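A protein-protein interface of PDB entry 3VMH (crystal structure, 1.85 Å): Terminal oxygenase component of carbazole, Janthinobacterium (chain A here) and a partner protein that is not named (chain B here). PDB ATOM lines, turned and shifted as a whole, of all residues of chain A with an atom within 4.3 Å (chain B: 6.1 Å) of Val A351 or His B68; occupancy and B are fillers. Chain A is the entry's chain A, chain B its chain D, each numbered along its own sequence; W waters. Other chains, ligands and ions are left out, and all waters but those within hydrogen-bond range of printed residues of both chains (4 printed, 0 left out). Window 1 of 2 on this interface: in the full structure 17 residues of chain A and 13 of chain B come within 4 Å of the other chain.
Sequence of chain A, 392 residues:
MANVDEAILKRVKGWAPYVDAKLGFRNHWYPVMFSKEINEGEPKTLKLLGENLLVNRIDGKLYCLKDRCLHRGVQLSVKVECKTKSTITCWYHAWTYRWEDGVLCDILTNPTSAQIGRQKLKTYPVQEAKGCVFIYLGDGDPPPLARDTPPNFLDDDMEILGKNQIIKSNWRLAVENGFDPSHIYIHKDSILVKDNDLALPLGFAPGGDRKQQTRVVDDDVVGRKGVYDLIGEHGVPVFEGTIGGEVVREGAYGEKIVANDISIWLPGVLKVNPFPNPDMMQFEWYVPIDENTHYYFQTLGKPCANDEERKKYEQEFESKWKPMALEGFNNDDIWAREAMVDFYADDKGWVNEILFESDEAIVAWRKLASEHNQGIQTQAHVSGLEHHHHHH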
ATOM      1  N   ILE A   8      30.867 -31.750 -28.803  1.00  0.00           N
ATOM      2  CA  ILE A   8      30.482 -30.375 -29.078  1.00  0.00           C
ATOM      3  C   ILE A   8      29.614 -30.336 -30.330  1.00  0.00           C
ATOM      4  O   ILE A   8      28.583 -29.670 -30.354  1.00  0.00           O
ATOM      5  CB  ILE A   8      31.723 -29.477 -29.263  1.00  0.00           C
ATOM      6  CG1 ILE A   8      32.475 -29.364 -27.929  1.00  0.00           C
ATOM      7  CG2 ILE A   8      31.307 -28.101 -29.764  1.00  0.00           C
ATOM      8  CD1 ILE A   8      33.822 -28.676 -28.029  1.00  0.00           C
ATOM      9  N   ARG A  11      26.033 -31.152 -29.811  1.00  0.00           N
ATOM     10  CA  ARG A  11      25.253 -30.103 -29.156  1.00  0.00           C
ATOM     11  C   ARG A  11      24.746 -29.005 -30.089  1.00  0.00           C
ATOM     12  O   ARG A  11      23.661 -28.468 -29.879  1.00  0.00           O
ATOM     13  CB  ARG A  11      26.078 -29.451 -28.043  1.00  0.00           C
ATOM     14  CG  ARG A  11      26.046 -30.172 -26.707  1.00  0.00           C
ATOM     15  CD  ARG A  11      27.058 -29.556 -25.751  1.00  0.00           C
ATOM     16  NE  ARG A  11      26.859 -30.007 -24.378  1.00  0.00           N
ATOM     17  CZ  ARG A  11      25.925 -29.530 -23.561  1.00  0.00           C
ATOM     18  NH1 ARG A  11      25.097 -28.576 -23.974  1.00  0.00           N
ATOM     19  NH2 ARG A  11      25.809 -30.018 -22.331  1.00  0.00           N
ATOM     20  N   LYS A 348      34.690 -24.248 -27.233  1.00  0.00           N
ATOM     21  CA  LYS A 348      33.620 -24.167 -26.239  1.00  0.00           C
ATOM     22  C   LYS A 348      32.727 -22.927 -26.365  1.00  0.00           C
ATOM     23  O   LYS A 348      31.595 -22.927 -25.884  1.00  0.00           O
ATOM     24  CB  LYS A 348      34.196 -24.237 -24.816  1.00  0.00           C
ATOM     25  CG  LYS A 348      34.921 -25.542 -24.485  1.00  0.00           C
ATOM     26  CD  LYS A 348      34.030 -26.758 -24.688  1.00  0.00           C
ATOM     27  CE  LYS A 348      34.806 -28.061 -24.480  1.00  0.00           C
ATOM     28  NZ  LYS A 348      35.363 -28.190 -23.105  1.00  0.00           N
ATOM     29  N   GLY A 349      33.239 -21.872 -26.995  1.00  0.00           N
ATOM     30  CA  GLY A 349      32.438 -20.669 -27.166  1.00  0.00           C
ATOM     31  C   GLY A 349      31.207 -20.929 -28.017  1.00  0.00           C
ATOM     32  O   GLY A 349      30.191 -20.241 -27.891  1.00  0.00           O
ATOM     33  N   TRP A 350      31.293 -21.928 -28.893  1.00  0.00           N
ATOM     34  CA  TRP A 350      30.181 -22.285 -29.770  1.00  0.00           C
ATOM     35  C   TRP A 350      29.013 -22.847 -28.973  1.00  0.00           C
ATOM     36  O   TRP A 350      27.903 -22.979 -29.496  1.00  0.00           O
ATOM     37  CB  TRP A 350      30.627 -23.312 -30.816  1.00  0.00           C
ATOM     38  CG  TRP A 350      31.720 -22.818 -31.702  1.00  0.00           C
ATOM     39  CD1 TRP A 350      33.011 -23.268 -31.745  1.00  0.00           C
ATOM     40  CD2 TRP A 350      31.623 -21.784 -32.683  1.00  0.00           C
ATOM     41  NE1 TRP A 350      33.724 -22.576 -32.695  1.00  0.00           N
ATOM     42  CE2 TRP A 350      32.895 -21.657 -33.285  1.00  0.00           C
ATOM     43  CE3 TRP A 350      30.582 -20.945 -33.114  1.00  0.00           C
ATOM     44  CZ2 TRP A 350      33.156 -20.727 -34.296  1.00  0.00           C
ATOM     45  CZ3 TRP A 350      30.842 -20.019 -34.120  1.00  0.00           C
ATOM     46  CH2 TRP A 350      32.121 -19.919 -34.698  1.00  0.00           C
ATOM     47  N   VAL A 351      29.264 -23.182 -27.711  1.00  0.00           N
ATOM     48  CA  VAL A 351      28.216 -23.709 -26.844  1.00  0.00           C
ATOM     49  C   VAL A 351      27.841 -22.701 -25.752  1.00  0.00           C
ATOM     50  O   VAL A 351      26.661 -22.517 -25.444  1.00  0.00           O
ATOM     51  CB  VAL A 351      28.663 -25.024 -26.147  1.00  0.00           C
ATOM     52  CG1 VAL A 351      27.610 -25.462 -25.135  1.00  0.00           C
ATOM     53  CG2 VAL A 351      28.881 -26.125 -27.182  1.00  0.00           C
ATOM     54  N   ASN A 352      28.848 -22.035 -25.194  1.00  0.00           N
ATOM     55  CA  ASN A 352      28.643 -21.098 -24.087  1.00  0.00           C
ATOM     56  C   ASN A 352      28.248 -19.649 -24.389  1.00  0.00           C
ATOM     57  O   ASN A 352      27.886 -18.900 -23.476  1.00  0.00           O
ATOM     58  CB  ASN A 352      29.878 -21.113 -23.189  1.00  0.00           C
ATOM     59  CG  ASN A 352      30.096 -22.459 -22.527  1.00  0.00           C
ATOM     60  OD1 ASN A 352      29.171 -23.031 -21.953  1.00  0.00           O
ATOM     61  ND2 ASN A 352      31.320 -22.971 -22.598  1.00  0.00           N
ATOM     62  N   GLU A 353      28.324 -19.254 -25.654  1.00  0.00           N
ATOM     63  CA  GLU A 353      27.948 -17.906 -26.063  1.00  0.00           C
ATOM     64  C   GLU A 353      26.485 -17.648 -25.674  1.00  0.00           C
ATOM     65  O   GLU A 353      25.663 -18.563 -25.718  1.00  0.00           O
ATOM     66  CB  GLU A 353      28.091 -17.785 -27.587  1.00  0.00           C
ATOM     67  CG  GLU A 353      27.286 -18.865 -28.325  1.00  0.00           C
ATOM     68  CD  GLU A 353      27.418 -18.829 -29.838  1.00  0.00           C
ATOM     69  OE1 GLU A 353      28.356 -18.192 -30.353  1.00  0.00           O
ATOM     70  OE2 GLU A 353      26.578 -19.465 -30.514  1.00  0.00           O
ATOM     71  N   HIS B  48      18.839 -19.123 -22.623  1.00  0.00           N
ATOM     72  CA  HIS B  48      20.274 -18.988 -22.861  1.00  0.00           C
ATOM     73  C   HIS B  48      20.588 -18.230 -24.155  1.00  0.00           C
ATOM     74  O   HIS B  48      21.741 -17.885 -24.419  1.00  0.00           O
ATOM     75  CB  HIS B  48      20.923 -20.380 -22.893  1.00  0.00           C
ATOM     76  CG  HIS B  48      22.388 -20.368 -23.214  1.00  0.00           C
ATOM     77  ND1 HIS B  48      22.884 -20.749 -24.443  1.00  0.00           N
ATOM     78  CD2 HIS B  48      23.465 -20.047 -22.458  1.00  0.00           C
ATOM     79  CE1 HIS B  48      24.203 -20.667 -24.428  1.00  0.00           C
ATOM     80  NE2 HIS B  48      24.581 -20.244 -23.235  1.00  0.00           N
ATOM     81  N   GLY B  49      19.565 -17.964 -24.961  1.00  0.00           N
ATOM     82  CA  GLY B  49      19.800 -17.259 -26.208  1.00  0.00           C
ATOM     83  C   GLY B  49      18.547 -16.774 -26.902  1.00  0.00           C
ATOM     84  O   GLY B  49      17.725 -16.076 -26.310  1.00  0.00           O
ATOM     85  N   CYS B  65      17.407 -27.781 -26.117  1.00  0.00           N
ATOM     86  CA  CYS B  65      17.511 -26.669 -27.056  1.00  0.00           C
ATOM     87  C   CYS B  65      18.361 -27.060 -28.268  1.00  0.00           C
ATOM     88  O   CYS B  65      19.440 -27.625 -28.118  1.00  0.00           O
ATOM     89  CB  CYS B  65      18.130 -25.458 -26.355  1.00  0.00           C
ATOM     90  SG  CYS B  65      18.385 -24.050 -27.441  1.00  0.00           S
ATOM     91  N   PRO B  66      17.884 -26.749 -29.486  1.00  0.00           N
ATOM     92  CA  PRO B  66      18.593 -27.069 -30.730  1.00  0.00           C
ATOM     93  C   PRO B  66      19.897 -26.306 -30.954  1.00  0.00           C
ATOM     94  O   PRO B  66      20.778 -26.768 -31.683  1.00  0.00           O
ATOM     95  CB  PRO B  66      17.547 -26.763 -31.802  1.00  0.00           C
ATOM     96  CG  PRO B  66      16.799 -25.617 -31.210  1.00  0.00           C
ATOM     97  CD  PRO B  66      16.614 -26.056 -29.773  1.00  0.00           C
ATOM     98  N   PHE B  67      20.024 -25.148 -30.313  1.00  0.00           N
ATOM     99  CA  PHE B  67      21.213 -24.317 -30.468  1.00  0.00           C
ATOM    100  C   PHE B  67      22.483 -24.863 -29.833  1.00  0.00           C
ATOM    101  O   PHE B  67      23.460 -25.149 -30.529  1.00  0.00           O
ATOM    102  CB  PHE B  67      20.953 -22.916 -29.902  1.00  0.00           C
ATOM    103  CG  PHE B  67      20.362 -21.950 -30.895  1.00  0.00           C
ATOM    104  CD1 PHE B  67      19.551 -22.394 -31.938  1.00  0.00           C
ATOM    105  CD2 PHE B  67      20.581 -20.582 -30.754  1.00  0.00           C
ATOM    106  CE1 PHE B  67      18.964 -21.483 -32.827  1.00  0.00           C
ATOM    107  CE2 PHE B  67      19.998 -19.667 -31.635  1.00  0.00           C
ATOM    108  CZ  PHE B  67      19.189 -20.119 -32.670  1.00  0.00           C
ATOM    109  N   HIS B  68      22.473 -25.008 -28.513  1.00  0.00           N
ATOM    110  CA  HIS B  68      23.668 -25.465 -27.819  1.00  0.00           C
ATOM    111  C   HIS B  68      23.515 -26.726 -26.987  1.00  0.00           C
ATOM    112  O   HIS B  68      24.454 -27.133 -26.311  1.00  0.00           O
ATOM    113  CB  HIS B  68      24.202 -24.332 -26.943  1.00  0.00           C
ATOM    114  CG  HIS B  68      24.323 -23.022 -27.660  1.00  0.00           C
ATOM    115  ND1 HIS B  68      23.492 -21.953 -27.404  1.00  0.00           N
ATOM    116  CD2 HIS B  68      25.173 -22.611 -28.633  1.00  0.00           C
ATOM    117  CE1 HIS B  68      23.822 -20.941 -28.186  1.00  0.00           C
ATOM    118  NE2 HIS B  68      24.840 -21.313 -28.942  1.00  0.00           N
ATOM    119  N   GLY B  69      22.342 -27.349 -27.028  1.00  0.00           N
ATOM    120  CA  GLY B  69      22.155 -28.572 -26.263  1.00  0.00           C
ATOM    121  C   GLY B  69      21.787 -28.372 -24.803  1.00  0.00           C
ATOM    122  O   GLY B  69      21.810 -29.325 -24.021  1.00  0.00           O
ATOM    123  N   GLY B  70      21.472 -27.138 -24.426  1.00  0.00           N
ATOM    124  CA  GLY B  70      21.059 -26.876 -23.058  1.00  0.00           C
ATOM    125  C   GLY B  70      19.680 -27.492 -22.906  1.00  0.00           C
ATOM    126  O   GLY B  70      19.031 -27.800 -23.910  1.00  0.00           O
ATOM    127  N   SER B  82      23.594 -28.050 -19.029  1.00  0.00           N
ATOM    128  CA  SER B  82      24.341 -26.832 -19.316  1.00  0.00           C
ATOM    129  C   SER B  82      24.177 -26.629 -20.825  1.00  0.00           C
ATOM    130  O   SER B  82      23.835 -27.572 -21.542  1.00  0.00           O
ATOM    131  CB  SER B  82      25.818 -27.022 -18.962  1.00  0.00           C
ATOM    132  OG  SER B  82      26.358 -28.147 -19.636  1.00  0.00           O
ATOM    133  N   PRO B  83      24.424 -25.408 -21.332  1.00  0.00           N
ATOM    134  CA  PRO B  83      24.852 -24.184 -20.645  1.00  0.00           C
ATOM    135  C   PRO B  83      23.742 -23.372 -19.971  1.00  0.00           C
ATOM    136  O   PRO B  83      24.012 -22.323 -19.382  1.00  0.00           O
ATOM    137  CB  PRO B  83      25.524 -23.394 -21.762  1.00  0.00           C
ATOM    138  CG  PRO B  83      24.625 -23.705 -22.937  1.00  0.00           C
ATOM    139  CD  PRO B  83      24.416 -25.212 -22.797  1.00  0.00           C
HETATM  140  O   HOH W   1      21.235 -29.551 -29.083  1.00  0.00           O
HETATM  141  O   HOH W   2      27.515 -27.391 -21.905  1.00  0.00           O
HETATM  142  O   HOH W   3      26.667 -19.937 -21.095  1.00  0.00           O
HETATM  143  O   HOH W   4      23.135 -18.213 -26.752  1.00  0.00           O
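The side-chain carboxylate of Glu A353 is in hydrogen-bond range of a ring nitrogen (NE2) of His B68 (3.0 Å).
The backbone carbonyl oxygen (O) of Ser B82 sits at hydrogen-bond distance from the guanidinium group (NH1) of Arg A11 (2.9 Å).
O of His B68 is in hydrogen-bond range of NH1 of Arg A11.
The backbone carbonyl oxygen (O) of Glu A353 lies close to a ring nitrogen (NE2) of His B48, 3.2 Å away.
O of Arg A11 sits close to O of Phe B67, 3.4 Å away.
N of Gly B69 lies within hydrogen-bond range of O of Arg A11 (3.3 Å).
O of Lys A348 is in hydrogen-bond range of ND2 of Asn A352.
SG of Cys B65 lies close to N of Phe B67 (3.5 Å).
O of Gly B70 is in hydrogen-bond range of N of Cys B65 (2.7 Å).
O of Pro B66 touches O of Arg A11, at 3.8 Å.
Arg A11 touches Gly B70.
Arg A11 touches Pro B83 (NH1 to CD, 3.6 Å).
His B68 touches Trp A350.
His B48 touches Val A351.
Val A351 touches His B68 (O to CG, 3.3 Å).
O of Val A351 touches CG of Pro B83 (3.4 Å).
His B48 touches Asn A352 (NE2 to O, 3.6 Å).
OD1 of Asn A352 touches CB of Pro B83, at 3.7 Å.
Printed residues of chain B within 4 Å of Arg A11: Pro B66 (3.8 Å), Phe B67 (3.4 Å), His B68 (2.8 Å), Gly B69 (3.3 Å), Gly B70 (3.9 Å), Ser B82 (2.9 Å) and Pro B83 (3.6 Å).
Printed residues of chain B within 4 Å of Trp A350: His B68 (2.9 Å).
Of the printed residues of chain B, Asn A352 touches His B48 and Pro B83.
Cys B65 touches none of the printed residues of chain A.
Printed residues of chain A within 4 Å of Pro B66: Arg A11.
His B68 touches just these residues of chain A: Arg A11 (2.8 Å), Trp A350 (2.9 Å), Val A351 (3.3 Å) and Glu A353 (3.0 Å).
The nearest residue of chain B that does not touch Val A351 is Ser B82 (5.6 Å).
Printed residues of chain A that touch a printed residue of chain B: Arg A11, Trp A350, Val A351, Asn A352 and Glu A353.
Hydrophobic or aromatic side chains of chain A that line the printed part of chain B: Val A351.
Hydrophobic or aromatic side chains of chain B that line the printed part of chain A: His B48, His B68 and Pro B83.
Among the printed residues, 15 pairs touch across the chains.
Water W2 bridges the side-chain hydroxyl of Ser B82 and the guanidinium group of Arg A11.
Water W4 bridges the backbone carbonyl oxygen of His B48 and the backbone carbonyl oxygen of Glu A353.
Water W1 lies within hydrogen-bond range of O of Arg A11 (2.8 Å), O of Cys B65 (2.8 Å) and N of Gly B69 (3.2 Å).
Water W3 lies within hydrogen-bond range of O of Asn A352 (2.9 Å) and NE2 of His B48 (3.0 Å).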
